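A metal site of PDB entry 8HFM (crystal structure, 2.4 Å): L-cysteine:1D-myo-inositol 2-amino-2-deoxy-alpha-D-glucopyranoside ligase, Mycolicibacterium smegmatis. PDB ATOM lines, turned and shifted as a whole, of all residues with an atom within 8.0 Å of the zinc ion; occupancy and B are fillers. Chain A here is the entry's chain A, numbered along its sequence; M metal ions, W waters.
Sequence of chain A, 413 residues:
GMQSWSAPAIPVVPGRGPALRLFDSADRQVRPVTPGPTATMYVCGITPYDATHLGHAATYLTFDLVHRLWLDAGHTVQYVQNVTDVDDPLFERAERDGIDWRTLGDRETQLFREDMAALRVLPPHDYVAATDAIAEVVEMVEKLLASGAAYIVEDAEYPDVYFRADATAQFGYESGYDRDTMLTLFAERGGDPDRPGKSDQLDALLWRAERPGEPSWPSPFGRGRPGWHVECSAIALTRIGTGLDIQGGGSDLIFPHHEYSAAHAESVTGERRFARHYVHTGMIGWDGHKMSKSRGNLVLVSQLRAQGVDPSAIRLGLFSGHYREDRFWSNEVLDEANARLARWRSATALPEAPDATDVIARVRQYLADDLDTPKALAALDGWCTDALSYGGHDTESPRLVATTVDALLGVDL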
ATOM      1  N   TYR A  42       9.340  -3.747 -17.090  1.00  0.00           N
ATOM      2  CA  TYR A  42       9.965  -4.608 -18.091  1.00  0.00           C
ATOM      3  C   TYR A  42       9.346  -5.991 -17.967  1.00  0.00           C
ATOM      4  O   TYR A  42       9.443  -6.621 -16.908  1.00  0.00           O
ATOM      5  CB  TYR A  42      11.473  -4.670 -17.884  1.00  0.00           C
ATOM      6  CG  TYR A  42      12.203  -5.448 -18.966  1.00  0.00           C
ATOM      7  CD1 TYR A  42      12.667  -4.804 -20.112  1.00  0.00           C
ATOM      8  CD2 TYR A  42      12.428  -6.818 -18.855  1.00  0.00           C
ATOM      9  CE1 TYR A  42      13.313  -5.491 -21.102  1.00  0.00           C
ATOM     10  CE2 TYR A  42      13.086  -7.523 -19.844  1.00  0.00           C
ATOM     11  CZ  TYR A  42      13.530  -6.854 -20.972  1.00  0.00           C
ATOM     12  OH  TYR A  42      14.177  -7.540 -21.962  1.00  0.00           O
ATOM     13  N   VAL A  43       8.686  -6.439 -19.029  1.00  0.00           N
ATOM     14  CA  VAL A  43       8.172  -7.806 -19.122  1.00  0.00           C
ATOM     15  C   VAL A  43       8.970  -8.514 -20.203  1.00  0.00           C
ATOM     16  O   VAL A  43       9.195  -7.960 -21.282  1.00  0.00           O
ATOM     17  CB  VAL A  43       6.671  -7.835 -19.414  1.00  0.00           C
ATOM     18  CG1 VAL A  43       6.172  -9.283 -19.493  1.00  0.00           C
ATOM     19  CG2 VAL A  43       5.917  -7.069 -18.353  1.00  0.00           C
ATOM     20  N   CYS A  44       9.411  -9.732 -19.902  1.00  0.00           N
ATOM     21  CA  CYS A  44      10.197 -10.482 -20.876  1.00  0.00           C
ATOM     22  C   CYS A  44       9.274 -10.959 -21.999  1.00  0.00           C
ATOM     23  O   CYS A  44       8.170 -11.447 -21.746  1.00  0.00           O
ATOM     24  CB  CYS A  44      10.894 -11.653 -20.196  1.00  0.00           C
ATOM     25  SG  CYS A  44      12.195 -11.142 -19.006  1.00  0.00           S
ATOM     26  N   GLY A  45       9.743 -10.813 -23.236  1.00  0.00           N
ATOM     27  CA  GLY A  45       8.931 -11.110 -24.391  1.00  0.00           C
ATOM     28  C   GLY A  45       8.957 -12.568 -24.785  1.00  0.00           C
ATOM     29  O   GLY A  45       9.243 -13.462 -23.979  1.00  0.00           O
ATOM     30  N   ILE A  46       8.647 -12.817 -26.053  1.00  0.00           N
ATOM     31  CA  ILE A  46       8.483 -14.155 -26.578  1.00  0.00           C
ATOM     32  C   ILE A  46       9.714 -14.549 -27.374  1.00  0.00           C
ATOM     33  O   ILE A  46      10.524 -13.712 -27.769  1.00  0.00           O
ATOM     34  CB  ILE A  46       7.219 -14.276 -27.465  1.00  0.00           C
ATOM     35  CG1 ILE A  46       7.297 -13.296 -28.638  1.00  0.00           C
ATOM     36  CG2 ILE A  46       5.949 -14.021 -26.639  1.00  0.00           C
ATOM     37  CD1 ILE A  46       7.040 -13.936 -29.977  1.00  0.00           C
ATOM     38  N   ASN A  82      10.814  -7.045 -24.812  1.00  0.00           N
ATOM     39  CA  ASN A  82      11.848  -7.483 -25.733  1.00  0.00           C
ATOM     40  C   ASN A  82      11.339  -8.606 -26.640  1.00  0.00           C
ATOM     41  O   ASN A  82      10.201  -9.086 -26.505  1.00  0.00           O
ATOM     42  CB  ASN A  82      13.080  -7.954 -24.953  1.00  0.00           C
ATOM     43  CG  ASN A  82      12.812  -9.258 -24.242  1.00  0.00           C
ATOM     44  OD1 ASN A  82      11.842  -9.360 -23.506  1.00  0.00           O
ATOM     45  ND2 ASN A  82      13.646 -10.257 -24.491  1.00  0.00           N
ATOM     46  N   VAL A  83      12.192  -9.028 -27.566  1.00  0.00           N
ATOM     47  CA  VAL A  83      11.989 -10.231 -28.382  1.00  0.00           C
ATOM     48  C   VAL A  83      13.306 -10.995 -28.404  1.00  0.00           C
ATOM     49  O   VAL A  83      14.325 -10.449 -28.858  1.00  0.00           O
ATOM     50  CB  VAL A  83      11.532  -9.904 -29.818  1.00  0.00           C
ATOM     51  CG1 VAL A  83      11.351 -11.177 -30.617  1.00  0.00           C
ATOM     52  CG2 VAL A  83      10.254  -9.094 -29.798  1.00  0.00           C
ATOM     53  N   THR A  84      13.298 -12.239 -27.938  1.00  0.00           N
ATOM     54  CA  THR A  84      14.521 -13.047 -27.860  1.00  0.00           C
ATOM     55  C   THR A  84      14.737 -13.746 -29.198  1.00  0.00           C
ATOM     56  O   THR A  84      14.411 -14.926 -29.392  1.00  0.00           O
ATOM     57  CB  THR A  84      14.434 -14.055 -26.715  1.00  0.00           C
ATOM     58  OG1 THR A  84      14.143 -13.375 -25.490  1.00  0.00           O
ATOM     59  CG2 THR A  84      15.765 -14.794 -26.569  1.00  0.00           C
ATOM     60  N   TRP A 228      21.803 -14.705 -22.740  1.00  0.00           N
ATOM     61  CA  TRP A 228      20.368 -14.431 -22.637  1.00  0.00           C
ATOM     62  C   TRP A 228      20.088 -13.391 -21.548  1.00  0.00           C
ATOM     63  O   TRP A 228      19.460 -12.354 -21.810  1.00  0.00           O
ATOM     64  CB  TRP A 228      19.601 -15.727 -22.358  1.00  0.00           C
ATOM     65  CG  TRP A 228      18.102 -15.577 -22.219  1.00  0.00           C
ATOM     66  CD1 TRP A 228      17.309 -14.567 -22.732  1.00  0.00           C
ATOM     67  CD2 TRP A 228      17.215 -16.464 -21.527  1.00  0.00           C
ATOM     68  NE1 TRP A 228      15.990 -14.787 -22.395  1.00  0.00           N
ATOM     69  CE2 TRP A 228      15.910 -15.947 -21.654  1.00  0.00           C
ATOM     70  CE3 TRP A 228      17.409 -17.646 -20.803  1.00  0.00           C
ATOM     71  CZ2 TRP A 228      14.798 -16.567 -21.093  1.00  0.00           C
ATOM     72  CZ3 TRP A 228      16.298 -18.277 -20.244  1.00  0.00           C
ATOM     73  CH2 TRP A 228      15.010 -17.734 -20.394  1.00  0.00           C
ATOM     74  N   HIS A 229      20.583 -13.639 -20.333  1.00  0.00           N
ATOM     75  CA  HIS A 229      20.198 -12.802 -19.191  1.00  0.00           C
ATOM     76  C   HIS A 229      20.735 -11.380 -19.306  1.00  0.00           C
ATOM     77  O   HIS A 229      20.075 -10.437 -18.868  1.00  0.00           O
ATOM     78  CB  HIS A 229      20.669 -13.437 -17.891  1.00  0.00           C
ATOM     79  CG  HIS A 229      20.654 -14.937 -17.911  1.00  0.00           C
ATOM     80  ND1 HIS A 229      19.531 -15.649 -18.272  1.00  0.00           N
ATOM     81  CD2 HIS A 229      21.604 -15.852 -17.631  1.00  0.00           C
ATOM     82  CE1 HIS A 229      19.798 -16.948 -18.212  1.00  0.00           C
ATOM     83  NE2 HIS A 229      21.047 -17.094 -17.816  1.00  0.00           N
ATOM     84  N   VAL A 230      21.915 -11.214 -19.899  1.00  0.00           N
ATOM     85  CA  VAL A 230      22.483  -9.876 -20.047  1.00  0.00           C
ATOM     86  C   VAL A 230      21.738  -9.076 -21.127  1.00  0.00           C
ATOM     87  O   VAL A 230      21.667  -7.846 -21.058  1.00  0.00           O
ATOM     88  CB  VAL A 230      24.004 -10.011 -20.314  1.00  0.00           C
ATOM     89  CG1 VAL A 230      24.287 -10.459 -21.732  1.00  0.00           C
ATOM     90  CG2 VAL A 230      24.716  -8.716 -20.038  1.00  0.00           C
ATOM     91  N   GLU A 231      21.128  -9.769 -22.112  1.00  0.00           N
ATOM     92  CA  GLU A 231      20.240  -9.083 -23.055  1.00  0.00           C
ATOM     93  C   GLU A 231      19.171  -8.286 -22.317  1.00  0.00           C
ATOM     94  O   GLU A 231      19.041  -7.068 -22.504  1.00  0.00           O
ATOM     95  CB  GLU A 231      19.588 -10.078 -24.013  1.00  0.00           C
ATOM     96  CG  GLU A 231      20.496 -10.585 -25.134  1.00  0.00           C
ATOM     97  CD  GLU A 231      19.993 -11.873 -25.798  1.00  0.00           C
ATOM     98  OE1 GLU A 231      18.755 -12.081 -25.879  1.00  0.00           O
ATOM     99  OE2 GLU A 231      20.840 -12.680 -26.228  1.00  0.00           O
ATOM    100  N   CYS A 232      18.396  -8.952 -21.460  1.00  0.00           N
ATOM    101  CA  CYS A 232      17.292  -8.277 -20.773  1.00  0.00           C
ATOM    102  C   CYS A 232      17.821  -7.272 -19.769  1.00  0.00           C
ATOM    103  O   CYS A 232      17.253  -6.178 -19.609  1.00  0.00           O
ATOM    104  CB  CYS A 232      16.401  -9.288 -20.067  1.00  0.00           C
ATOM    105  SG  CYS A 232      15.442 -10.236 -21.196  1.00  0.00           S
ATOM    106  N   SER A 233      18.897  -7.632 -19.090  1.00  0.00           N
ATOM    107  CA  SER A 233      19.480  -6.743 -18.085  1.00  0.00           C
ATOM    108  C   SER A 233      19.918  -5.432 -18.738  1.00  0.00           C
ATOM    109  O   SER A 233      19.700  -4.352 -18.176  1.00  0.00           O
ATOM    110  CB  SER A 233      20.635  -7.467 -17.410  1.00  0.00           C
ATOM    111  OG  SER A 233      21.054  -6.799 -16.237  1.00  0.00           O
ATOM    112  N   ILE A 235      18.835  -4.114 -21.804  1.00  0.00           N
ATOM    113  CA  ILE A 235      17.709  -3.358 -22.358  1.00  0.00           C
ATOM    114  C   ILE A 235      17.004  -2.579 -21.257  1.00  0.00           C
ATOM    115  O   ILE A 235      16.769  -1.371 -21.384  1.00  0.00           O
ATOM    116  CB  ILE A 235      16.750  -4.304 -23.092  1.00  0.00           C
ATOM    117  CG1 ILE A 235      17.465  -4.930 -24.295  1.00  0.00           C
ATOM    118  CG2 ILE A 235      15.472  -3.572 -23.509  1.00  0.00           C
ATOM    119  CD1 ILE A 235      16.717  -6.084 -24.904  1.00  0.00           C
ATOM    120  N   GLN A 247       9.855  -6.100 -12.651  1.00  0.00           N
ATOM    121  CA  GLN A 247      10.373  -7.073 -13.587  1.00  0.00           C
ATOM    122  C   GLN A 247       9.356  -8.203 -13.675  1.00  0.00           C
ATOM    123  O   GLN A 247       9.007  -8.808 -12.656  1.00  0.00           O
ATOM    124  CB  GLN A 247      11.747  -7.593 -13.140  1.00  0.00           C
ATOM    125  CG  GLN A 247      12.159  -8.904 -13.767  1.00  0.00           C
ATOM    126  CD  GLN A 247      12.553  -8.768 -15.212  1.00  0.00           C
ATOM    127  OE1 GLN A 247      13.666  -8.374 -15.528  1.00  0.00           O
ATOM    128  NE2 GLN A 247      11.626  -9.095 -16.122  1.00  0.00           N
ATOM    129  N   GLY A 248       8.877  -8.482 -14.876  1.00  0.00           N
ATOM    130  CA  GLY A 248       7.773  -9.403 -15.049  1.00  0.00           C
ATOM    131  C   GLY A 248       8.070 -10.535 -16.007  1.00  0.00           C
ATOM    132  O   GLY A 248       8.922 -10.423 -16.898  1.00  0.00           O
ATOM    133  N   GLY A 249       7.336 -11.614 -15.824  1.00  0.00           N
ATOM    134  CA  GLY A 249       7.349 -12.703 -16.775  1.00  0.00           C
ATOM    135  C   GLY A 249       6.756 -13.950 -16.153  1.00  0.00           C
ATOM    136  O   GLY A 249       6.293 -13.944 -15.009  1.00  0.00           O
ATOM    137  N   LEU A 253      10.852 -18.176 -15.568  1.00  0.00           N
ATOM    138  CA  LEU A 253      11.921 -17.189 -15.589  1.00  0.00           C
ATOM    139  C   LEU A 253      12.468 -16.839 -14.206  1.00  0.00           C
ATOM    140  O   LEU A 253      13.448 -16.078 -14.120  1.00  0.00           O
ATOM    141  CB  LEU A 253      11.442 -15.906 -16.287  1.00  0.00           C
ATOM    142  CG  LEU A 253      10.819 -16.093 -17.682  1.00  0.00           C
ATOM    143  CD1 LEU A 253      10.439 -14.751 -18.317  1.00  0.00           C
ATOM    144  CD2 LEU A 253      11.746 -16.881 -18.593  1.00  0.00           C
ATOM    145  N   HIS A 257      16.699 -17.125 -15.218  1.00  0.00           N
ATOM    146  CA  HIS A 257      16.716 -15.915 -16.037  1.00  0.00           C
ATOM    147  C   HIS A 257      16.680 -14.646 -15.195  1.00  0.00           C
ATOM    148  O   HIS A 257      17.509 -13.758 -15.354  1.00  0.00           O
ATOM    149  CB  HIS A 257      15.561 -15.909 -17.029  1.00  0.00           C
ATOM    150  CG  HIS A 257      15.690 -14.827 -18.042  1.00  0.00           C
ATOM    151  ND1 HIS A 257      16.850 -14.622 -18.743  1.00  0.00           N
ATOM    152  CD2 HIS A 257      14.819 -13.870 -18.439  1.00  0.00           C
ATOM    153  CE1 HIS A 257      16.692 -13.588 -19.561  1.00  0.00           C
ATOM    154  NE2 HIS A 257      15.470 -13.120 -19.390  1.00  0.00           N
ATOM    155  N   HIS A 258      15.682 -14.522 -14.319  1.00  0.00           N
ATOM    156  CA  HIS A 258      15.561 -13.252 -13.600  1.00  0.00           C
ATOM    157  C   HIS A 258      16.554 -13.132 -12.453  1.00  0.00           C
ATOM    158  O   HIS A 258      16.879 -12.014 -12.055  1.00  0.00           O
ATOM    159  CB  HIS A 258      14.115 -13.079 -13.101  1.00  0.00           C
ATOM    160  CG  HIS A 258      13.147 -12.764 -14.198  1.00  0.00           C
ATOM    161  ND1 HIS A 258      11.801 -13.014 -14.109  1.00  0.00           N
ATOM    162  CD2 HIS A 258      13.349 -12.209 -15.423  1.00  0.00           C
ATOM    163  CE1 HIS A 258      11.205 -12.637 -15.222  1.00  0.00           C
ATOM    164  NE2 HIS A 258      12.121 -12.149 -16.037  1.00  0.00           N
ATOM    165  N   SER A 261      19.752 -11.992 -14.508  1.00  0.00           N
ATOM    166  CA  SER A 261      19.513 -10.679 -15.079  1.00  0.00           C
ATOM    167  C   SER A 261      19.505  -9.603 -13.989  1.00  0.00           C
ATOM    168  O   SER A 261      20.033  -8.508 -14.197  1.00  0.00           O
ATOM    169  CB  SER A 261      18.216 -10.682 -15.874  1.00  0.00           C
ATOM    170  OG  SER A 261      17.717  -9.374 -16.033  1.00  0.00           O
HETATM  171 ZN    ZN M   1      13.971 -11.728 -20.307  1.00  0.00          ZN
HETATM  172  O   HOH W   1      13.405 -12.690 -22.285  1.00  0.00           O
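A ring nitrogen (ND1) of His 257 lies within hydrogen-bond range of a ring nitrogen (ND1) of His 229 (2.9 Å). A ring nitrogen (NE2) of His 258 sits close to the side-chain sulfur of Cys 44 (3.1 Å). SG of Cys 44 sits close to NE2 of Gln 247, 3.6 Å away. The side-chain sulfur (SG) of Cys 232 sits close to the side-chain amide nitrogen (ND2) of Asn 82 (3.8 Å). The backbone NH (N) of Cys 44 lies within hydrogen-bond range of the backbone carbonyl oxygen (O) of Gly 248 (3.1 Å). A ring nitrogen (NE2) of His 257 sits close to the indole nitrogen (NE1) of Trp 228, at 3.5 Å. SG of Cys 232 lies close to OH of Tyr 42.
The nearest printed residue that does not touch the zinc ion is Trp 228 (4.2 Å).
The zinc ion is bound by NE2 of His 257 (2.2 Å). The zinc ion is bound by water W1. SG of Cys 232 is bound to the zinc ion (2.3 Å). SG of Cys 44 is bound to the zinc ion (2.3 Å). The zinc ion has four donor atoms within binding distance.
Water W1 lies within hydrogen-bond range of ND2 of Asn 82, NE1 of Trp 228 and OG1 of Thr 84.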
